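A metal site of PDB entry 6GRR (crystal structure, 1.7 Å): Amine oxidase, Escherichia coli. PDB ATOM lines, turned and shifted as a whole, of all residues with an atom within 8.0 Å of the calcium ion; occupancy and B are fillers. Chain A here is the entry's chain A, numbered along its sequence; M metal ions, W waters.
The side-chain carboxylate of Asp 529 is in hydrogen-bond range of the indole nitrogen of Trp 131 (2.8 Å). The backbone carbonyl oxygen (O) of Glu 353 lies within hydrogen-bond range of the backbone NH (N) of Asp 527 (2.8 Å). NZ of Lys 127 lies within salt-bridge range of OD2 of Asp 529. The side-chain amino group of Lys 127 is in salt-bridge range of the side-chain carboxylate of Asp 672, 2.7 Å away. N of Tyr 637 lies within hydrogen-bond range of O of Asp 672, at 2.9 Å. O of Val 350 lies within hydrogen-bond range of N of Asp 529 (3.0 Å). The side-chain carboxylate (OD2) of Asp 527 is in salt-bridge range of the side-chain amino group (NZ) of Lys 127. The backbone NH of Tyr 352 lies within hydrogen-bond range of the backbone carbonyl oxygen of Asp 527 (2.8 Å).
Water W1 lies within hydrogen-bond range of O of Glu 533 (2.6 Å), OD1 of Asn 535 (2.9 Å) and N of Ala 673 (3.0 Å).
OD1 of Asp 529 binds the calcium ion. The calcium ion is bound by OD1 of Asp 672 (2.3 Å). The backbone carbonyl oxygen (O) of Ala 673 binds the calcium ion, at 2.3 Å. OD1 of Asp 527 binds the calcium ion. O of Leu 528 is bound to the calcium ion, 2.3 Å away. Water W1 is bound to the calcium ion, at 2.4 Å. The calcium ion has six donor atoms within binding distance.
Merely in contact with the calcium ion: Lys 127 (3.8 Å). Of the 25 residues printed, 6 come within 4 Å of the calcium ion. The nearest printed residue that does not touch the calcium ion is Glu 533 (4.5 Å).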
ATOM      1  N   LYS A 127     -12.433 -14.707   1.097  1.00  0.00           N
ATOM      2  CA  LYS A 127     -11.043 -14.837   0.728  1.00  0.00           C
ATOM      3  C   LYS A 127     -10.708 -14.051  -0.552  1.00  0.00           C
ATOM      4  O   LYS A 127      -9.706 -13.355  -0.619  1.00  0.00           O
ATOM      5  CB  LYS A 127     -10.718 -16.313   0.544  1.00  0.00           C
ATOM      6  CG  LYS A 127      -9.376 -16.593  -0.093  1.00  0.00           C
ATOM      7  CD  LYS A 127      -9.085 -18.073  -0.025  1.00  0.00           C
ATOM      8  CE  LYS A 127      -7.733 -18.361  -0.646  1.00  0.00           C
ATOM      9  NZ  LYS A 127      -7.274 -19.735  -0.385  1.00  0.00           N
ATOM     10  N   TRP A 131      -7.823 -11.098  -0.746  1.00  0.00           N
ATOM     11  CA  TRP A 131      -6.695 -11.083  -1.650  1.00  0.00           C
ATOM     12  C   TRP A 131      -6.701  -9.839  -2.539  1.00  0.00           C
ATOM     13  O   TRP A 131      -5.647  -9.267  -2.795  1.00  0.00           O
ATOM     14  CB  TRP A 131      -6.631 -12.316  -2.564  1.00  0.00           C
ATOM     15  CG  TRP A 131      -5.803 -13.454  -2.077  1.00  0.00           C
ATOM     16  CD1 TRP A 131      -6.176 -14.755  -2.038  1.00  0.00           C
ATOM     17  CD2 TRP A 131      -4.433 -13.412  -1.672  1.00  0.00           C
ATOM     18  NE1 TRP A 131      -5.132 -15.535  -1.580  1.00  0.00           N
ATOM     19  CE2 TRP A 131      -4.051 -14.732  -1.345  1.00  0.00           C
ATOM     20  CE3 TRP A 131      -3.497 -12.387  -1.513  1.00  0.00           C
ATOM     21  CZ2 TRP A 131      -2.788 -15.060  -0.882  1.00  0.00           C
ATOM     22  CZ3 TRP A 131      -2.226 -12.705  -1.038  1.00  0.00           C
ATOM     23  CH2 TRP A 131      -1.889 -14.042  -0.743  1.00  0.00           C
ATOM     24  N   VAL A 350       1.760 -16.648  -1.985  1.00  0.00           N
ATOM     25  CA  VAL A 350       2.331 -17.843  -1.404  1.00  0.00           C
ATOM     26  C   VAL A 350       1.353 -18.482  -0.428  1.00  0.00           C
ATOM     27  O   VAL A 350       1.133 -19.688  -0.501  1.00  0.00           O
ATOM     28  CB  VAL A 350       3.681 -17.555  -0.702  1.00  0.00           C
ATOM     29  CG1 VAL A 350       4.201 -18.787   0.023  1.00  0.00           C
ATOM     30  CG2 VAL A 350       4.724 -17.051  -1.685  1.00  0.00           C
ATOM     31  N   MET A 351       0.799 -17.724   0.512  1.00  0.00           N
ATOM     32  CA  MET A 351      -0.092 -18.287   1.523  1.00  0.00           C
ATOM     33  C   MET A 351      -1.198 -17.331   1.934  1.00  0.00           C
ATOM     34  O   MET A 351      -0.933 -16.197   2.355  1.00  0.00           O
ATOM     35  CB  MET A 351       0.734 -18.750   2.750  1.00  0.00           C
ATOM     36  CG  MET A 351      -0.088 -19.427   3.800  1.00  0.00           C
ATOM     37  SD  MET A 351       0.898 -20.204   5.112  1.00  0.00           S
ATOM     38  CE  MET A 351       1.583 -18.753   5.858  1.00  0.00           C
ATOM     39  N   TYR A 352      -2.469 -17.762   1.806  1.00  0.00           N
ATOM     40  CA  TYR A 352      -3.573 -16.952   2.256  1.00  0.00           C
ATOM     41  C   TYR A 352      -3.646 -16.841   3.745  1.00  0.00           C
ATOM     42  O   TYR A 352      -3.793 -15.744   4.253  1.00  0.00           O
ATOM     43  CB  TYR A 352      -4.915 -17.411   1.654  1.00  0.00           C
ATOM     44  CG  TYR A 352      -6.044 -16.558   2.104  1.00  0.00           C
ATOM     45  CD1 TYR A 352      -6.118 -15.215   1.723  1.00  0.00           C
ATOM     46  CD2 TYR A 352      -7.029 -17.047   2.954  1.00  0.00           C
ATOM     47  CE1 TYR A 352      -7.112 -14.386   2.203  1.00  0.00           C
ATOM     48  CE2 TYR A 352      -8.042 -16.227   3.429  1.00  0.00           C
ATOM     49  CZ  TYR A 352      -8.085 -14.903   3.058  1.00  0.00           C
ATOM     50  OH  TYR A 352      -9.084 -14.098   3.542  1.00  0.00           O
ATOM     51  N   GLU A 353      -3.567 -17.957   4.460  1.00  0.00           N
ATOM     52  CA  GLU A 353      -3.617 -17.954   5.916  1.00  0.00           C
ATOM     53  C   GLU A 353      -2.827 -19.157   6.393  1.00  0.00           C
ATOM     54  O   GLU A 353      -2.991 -20.274   5.852  1.00  0.00           O
ATOM     55  CB  GLU A 353      -5.054 -18.132   6.453  1.00  0.00           C
ATOM     56  CG  GLU A 353      -5.950 -16.934   6.273  1.00  0.00           C
ATOM     57  CD  GLU A 353      -7.386 -17.188   6.743  1.00  0.00           C
ATOM     58  OE1 GLU A 353      -8.081 -18.134   6.279  1.00  0.00           O
ATOM     59  OE2 GLU A 353      -7.837 -16.398   7.583  1.00  0.00           O
ATOM     60  N   ARG A 525      -2.038 -25.554  10.097  1.00  0.00           N
ATOM     61  CA  ARG A 525      -2.980 -25.364   8.982  1.00  0.00           C
ATOM     62  C   ARG A 525      -2.432 -24.287   8.094  1.00  0.00           C
ATOM     63  O   ARG A 525      -2.283 -23.112   8.533  1.00  0.00           O
ATOM     64  CB  ARG A 525      -4.346 -24.953   9.533  1.00  0.00           C
ATOM     65  CG  ARG A 525      -5.378 -24.719   8.435  1.00  0.00           C
ATOM     66  CD  ARG A 525      -6.691 -24.128   8.969  1.00  0.00           C
ATOM     67  NE  ARG A 525      -7.617 -23.865   7.857  1.00  0.00           N
ATOM     68  CZ  ARG A 525      -7.533 -22.852   6.997  1.00  0.00           C
ATOM     69  NH1 ARG A 525      -6.611 -21.893   7.117  1.00  0.00           N
ATOM     70  NH2 ARG A 525      -8.431 -22.776   6.016  1.00  0.00           N
ATOM     71  N   LEU A 526      -2.142 -24.656   6.851  1.00  0.00           N
ATOM     72  CA  LEU A 526      -1.439 -23.790   5.923  1.00  0.00           C
ATOM     73  C   LEU A 526      -2.203 -23.717   4.609  1.00  0.00           C
ATOM     74  O   LEU A 526      -2.058 -24.608   3.743  1.00  0.00           O
ATOM     75  CB  LEU A 526      -0.039 -24.320   5.663  1.00  0.00           C
ATOM     76  CG  LEU A 526       0.794 -24.536   6.949  1.00  0.00           C
ATOM     77  CD1 LEU A 526       2.056 -25.321   6.607  1.00  0.00           C
ATOM     78  CD2 LEU A 526       1.128 -23.210   7.595  1.00  0.00           C
ATOM     79  N   ASP A 527      -3.007 -22.661   4.465  1.00  0.00           N
ATOM     80  CA  ASP A 527      -3.722 -22.422   3.194  1.00  0.00           C
ATOM     81  C   ASP A 527      -2.770 -21.769   2.217  1.00  0.00           C
ATOM     82  O   ASP A 527      -2.835 -20.563   1.967  1.00  0.00           O
ATOM     83  CB  ASP A 527      -4.973 -21.594   3.436  1.00  0.00           C
ATOM     84  CG  ASP A 527      -5.756 -21.312   2.153  1.00  0.00           C
ATOM     85  OD1 ASP A 527      -5.474 -21.946   1.126  1.00  0.00           O
ATOM     86  OD2 ASP A 527      -6.640 -20.473   2.219  1.00  0.00           O
ATOM     87  N   LEU A 528      -1.863 -22.588   1.680  1.00  0.00           N
ATOM     88  CA  LEU A 528      -0.954 -22.162   0.613  1.00  0.00           C
ATOM     89  C   LEU A 528      -1.781 -21.917  -0.649  1.00  0.00           C
ATOM     90  O   LEU A 528      -2.682 -22.685  -0.916  1.00  0.00           O
ATOM     91  CB  LEU A 528       0.096 -23.229   0.322  1.00  0.00           C
ATOM     92  CG  LEU A 528       0.977 -23.608   1.519  1.00  0.00           C
ATOM     93  CD1 LEU A 528       1.941 -24.717   1.144  1.00  0.00           C
ATOM     94  CD2 LEU A 528       1.698 -22.381   2.022  1.00  0.00           C
ATOM     95  N   ASP A 529      -1.519 -20.812  -1.328  1.00  0.00           N
ATOM     96  CA  ASP A 529      -2.052 -20.497  -2.637  1.00  0.00           C
ATOM     97  C   ASP A 529      -0.769 -20.259  -3.445  1.00  0.00           C
ATOM     98  O   ASP A 529      -0.173 -19.172  -3.376  1.00  0.00           O
ATOM     99  CB  ASP A 529      -2.898 -19.220  -2.587  1.00  0.00           C
ATOM    100  CG  ASP A 529      -4.281 -19.412  -1.964  1.00  0.00           C
ATOM    101  OD1 ASP A 529      -4.726 -20.541  -1.686  1.00  0.00           O
ATOM    102  OD2 ASP A 529      -4.930 -18.356  -1.752  1.00  0.00           O
ATOM    103  N   VAL A 530      -0.311 -21.300  -4.136  1.00  0.00           N
ATOM    104  CA  VAL A 530       1.014 -21.259  -4.775  1.00  0.00           C
ATOM    105  C   VAL A 530       0.883 -20.472  -6.094  1.00  0.00           C
ATOM    106  O   VAL A 530       0.460 -21.027  -7.110  1.00  0.00           O
ATOM    107  CB  VAL A 530       1.587 -22.657  -5.000  1.00  0.00           C
ATOM    108  CG1 VAL A 530       2.914 -22.592  -5.744  1.00  0.00           C
ATOM    109  CG2 VAL A 530       1.797 -23.358  -3.647  1.00  0.00           C
ATOM    110  N   GLY A 532      -1.259 -18.476  -6.866  1.00  0.00           N
ATOM    111  CA  GLY A 532      -2.650 -18.587  -7.281  1.00  0.00           C
ATOM    112  C   GLY A 532      -3.409 -19.577  -6.460  1.00  0.00           C
ATOM    113  O   GLY A 532      -2.820 -20.425  -5.787  1.00  0.00           O
ATOM    114  N   GLU A 533      -4.728 -19.478  -6.553  1.00  0.00           N
ATOM    115  CA  GLU A 533      -5.690 -20.329  -5.879  1.00  0.00           C
ATOM    116  C   GLU A 533      -5.598 -21.800  -6.289  1.00  0.00           C
ATOM    117  O   GLU A 533      -5.574 -22.727  -5.453  1.00  0.00           O
ATOM    118  CB  GLU A 533      -7.092 -19.793  -6.223  1.00  0.00           C
ATOM    119  CG  GLU A 533      -8.262 -20.490  -5.571  1.00  0.00           C
ATOM    120  CD  GLU A 533      -9.617 -20.049  -6.136  1.00  0.00           C
ATOM    121  OE1 GLU A 533      -9.674 -19.078  -6.928  1.00  0.00           O
ATOM    122  OE2 GLU A 533     -10.636 -20.670  -5.772  1.00  0.00           O
ATOM    123  N   ASN A 534      -5.575 -22.015  -7.580  1.00  0.00           N
ATOM    124  CA  ASN A 534      -5.793 -23.347  -8.134  1.00  0.00           C
ATOM    125  C   ASN A 534      -4.490 -24.116  -8.236  1.00  0.00           C
ATOM    126  O   ASN A 534      -3.623 -23.754  -9.013  1.00  0.00           O
ATOM    127  CB  ASN A 534      -6.476 -23.206  -9.490  1.00  0.00           C
ATOM    128  CG  ASN A 534      -7.883 -22.661  -9.347  1.00  0.00           C
ATOM    129  OD1 ASN A 534      -8.625 -23.098  -8.468  1.00  0.00           O
ATOM    130  ND2 ASN A 534      -8.239 -21.707 -10.165  1.00  0.00           N
ATOM    131  N   ASN A 535      -4.380 -25.136  -7.387  1.00  0.00           N
ATOM    132  CA  ASN A 535      -3.181 -25.931  -7.204  1.00  0.00           C
ATOM    133  C   ASN A 535      -3.517 -27.441  -7.245  1.00  0.00           C
ATOM    134  O   ASN A 535      -4.702 -27.844  -7.193  1.00  0.00           O
ATOM    135  CB  ASN A 535      -2.507 -25.607  -5.846  1.00  0.00           C
ATOM    136  CG  ASN A 535      -2.085 -24.152  -5.669  1.00  0.00           C
ATOM    137  OD1 ASN A 535      -1.876 -23.753  -4.507  1.00  0.00           O
ATOM    138  ND2 ASN A 535      -1.911 -23.359  -6.752  1.00  0.00           N
ATOM    139  N   LEU A 582       3.059 -28.866  -3.574  1.00  0.00           N
ATOM    140  CA  LEU A 582       1.831 -28.194  -4.009  1.00  0.00           C
ATOM    141  C   LEU A 582       2.203 -27.341  -5.200  1.00  0.00           C
ATOM    142  O   LEU A 582       2.960 -26.379  -5.077  1.00  0.00           O
ATOM    143  CB  LEU A 582       1.211 -27.371  -2.877  1.00  0.00           C
ATOM    144  CG  LEU A 582      -0.230 -26.949  -3.101  1.00  0.00           C
ATOM    145  CD1 LEU A 582      -1.162 -28.164  -3.192  1.00  0.00           C
ATOM    146  CD2 LEU A 582      -0.675 -26.011  -2.006  1.00  0.00           C
ATOM    147  N   THR A 635      -6.729 -30.712   1.960  1.00  0.00           N
ATOM    148  CA  THR A 635      -8.187 -30.621   1.885  1.00  0.00           C
ATOM    149  C   THR A 635      -8.567 -29.493   0.967  1.00  0.00           C
ATOM    150  O   THR A 635      -7.715 -28.690   0.584  1.00  0.00           O
ATOM    151  CB  THR A 635      -8.833 -30.461   3.272  1.00  0.00           C
ATOM    152  OG1 THR A 635      -8.357 -29.266   3.914  1.00  0.00           O
ATOM    153  CG2 THR A 635      -8.565 -31.673   4.128  1.00  0.00           C
ATOM    154  N   ARG A 636      -9.824 -29.450   0.559  1.00  0.00           N
ATOM    155  CA  ARG A 636     -10.342 -28.319  -0.206  1.00  0.00           C
ATOM    156  C   ARG A 636     -10.630 -27.161   0.747  1.00  0.00           C
ATOM    157  O   ARG A 636     -11.152 -27.364   1.840  1.00  0.00           O
ATOM    158  CB  ARG A 636     -11.613 -28.710  -0.986  1.00  0.00           C
ATOM    159  CG  ARG A 636     -11.342 -29.789  -2.017  1.00  0.00           C
ATOM    160  CD  ARG A 636     -12.638 -30.305  -2.639  1.00  0.00           C
ATOM    161  NE  ARG A 636     -13.374 -29.245  -3.316  1.00  0.00           N
ATOM    162  CZ  ARG A 636     -13.285 -28.900  -4.616  1.00  0.00           C
ATOM    163  NH1 ARG A 636     -12.486 -29.538  -5.481  1.00  0.00           N
ATOM    164  NH2 ARG A 636     -14.040 -27.908  -5.044  1.00  0.00           N
ATOM    165  N   TYR A 637     -10.263 -25.939   0.334  1.00  0.00           N
ATOM    166  CA  TYR A 637     -10.517 -24.746   1.116  1.00  0.00           C
ATOM    167  C   TYR A 637     -11.991 -24.617   1.537  1.00  0.00           C
ATOM    168  O   TYR A 637     -12.887 -24.657   0.675  1.00  0.00           O
ATOM    169  CB  TYR A 637     -10.147 -23.476   0.350  1.00  0.00           C
ATOM    170  CG  TYR A 637     -10.547 -22.203   1.086  1.00  0.00           C
ATOM    171  CD1 TYR A 637      -9.904 -21.818   2.262  1.00  0.00           C
ATOM    172  CD2 TYR A 637     -11.621 -21.419   0.636  1.00  0.00           C
ATOM    173  CE1 TYR A 637     -10.282 -20.683   2.963  1.00  0.00           C
ATOM    174  CE2 TYR A 637     -11.996 -20.273   1.328  1.00  0.00           C
ATOM    175  CZ  TYR A 637     -11.342 -19.918   2.494  1.00  0.00           C
ATOM    176  OH  TYR A 637     -11.740 -18.792   3.190  1.00  0.00           O
ATOM    177  N   THR A 671      -7.363 -26.951  -7.832  1.00  0.00           N
ATOM    178  CA  THR A 671      -8.391 -26.337  -7.015  1.00  0.00           C
ATOM    179  C   THR A 671      -7.730 -25.734  -5.776  1.00  0.00           C
ATOM    180  O   THR A 671      -6.521 -25.898  -5.568  1.00  0.00           O
ATOM    181  CB  THR A 671      -9.502 -27.372  -6.666  1.00  0.00           C
ATOM    182  OG1 THR A 671     -10.656 -26.703  -6.141  1.00  0.00           O
ATOM    183  CG2 THR A 671      -9.026 -28.409  -5.657  1.00  0.00           C
ATOM    184  N   ASP A 672      -8.514 -25.006  -4.990  1.00  0.00           N
ATOM    185  CA  ASP A 672      -7.995 -24.328  -3.803  1.00  0.00           C
ATOM    186  C   ASP A 672      -7.766 -25.356  -2.697  1.00  0.00           C
ATOM    187  O   ASP A 672      -8.724 -25.902  -2.139  1.00  0.00           O
ATOM    188  CB  ASP A 672      -8.944 -23.222  -3.349  1.00  0.00           C
ATOM    189  CG  ASP A 672      -8.310 -22.304  -2.291  1.00  0.00           C
ATOM    190  OD1 ASP A 672      -7.192 -22.644  -1.794  1.00  0.00           O
ATOM    191  OD2 ASP A 672      -8.916 -21.259  -1.971  1.00  0.00           O
ATOM    192  N   ALA A 673      -6.498 -25.621  -2.424  1.00  0.00           N
ATOM    193  CA  ALA A 673      -6.102 -26.598  -1.424  1.00  0.00           C
ATOM    194  C   ALA A 673      -5.631 -25.940  -0.139  1.00  0.00           C
ATOM    195  O   ALA A 673      -5.092 -24.826  -0.187  1.00  0.00           O
ATOM    196  CB  ALA A 673      -4.992 -27.464  -1.972  1.00  0.00           C
ATOM    197  N   VAL A 674      -5.743 -26.694   0.950  1.00  0.00           N
ATOM    198  CA  VAL A 674      -5.224 -26.327   2.261  1.00  0.00           C
ATOM    199  C   VAL A 674      -4.371 -27.511   2.733  1.00  0.00           C
ATOM    200  O   VAL A 674      -4.807 -28.671   2.743  1.00  0.00           O
ATOM    201  CB  VAL A 674      -6.360 -26.024   3.269  1.00  0.00           C
ATOM    202  CG1 VAL A 674      -5.814 -25.744   4.673  1.00  0.00           C
ATOM    203  CG2 VAL A 674      -7.223 -24.857   2.808  1.00  0.00           C
ATOM    204  N   VAL A 675      -3.131 -27.207   3.112  1.00  0.00           N
ATOM    205  CA  VAL A 675      -2.198 -28.196   3.571  1.00  0.00           C
ATOM    206  C   VAL A 675      -2.205 -28.212   5.094  1.00  0.00           C
ATOM    207  O   VAL A 675      -2.216 -27.156   5.714  1.00  0.00           O
ATOM    208  CB  VAL A 675      -0.796 -27.856   3.037  1.00  0.00           C
ATOM    209  CG1 VAL A 675       0.258 -28.766   3.667  1.00  0.00           C
ATOM    210  CG2 VAL A 675      -0.780 -27.987   1.510  1.00  0.00           C
HETATM  211 CA    CA M   1      -5.021 -22.674  -1.029  1.00  0.00          CA
HETATM  212  O   HOH W   1      -4.446 -23.576  -3.222  1.00  0.00           O
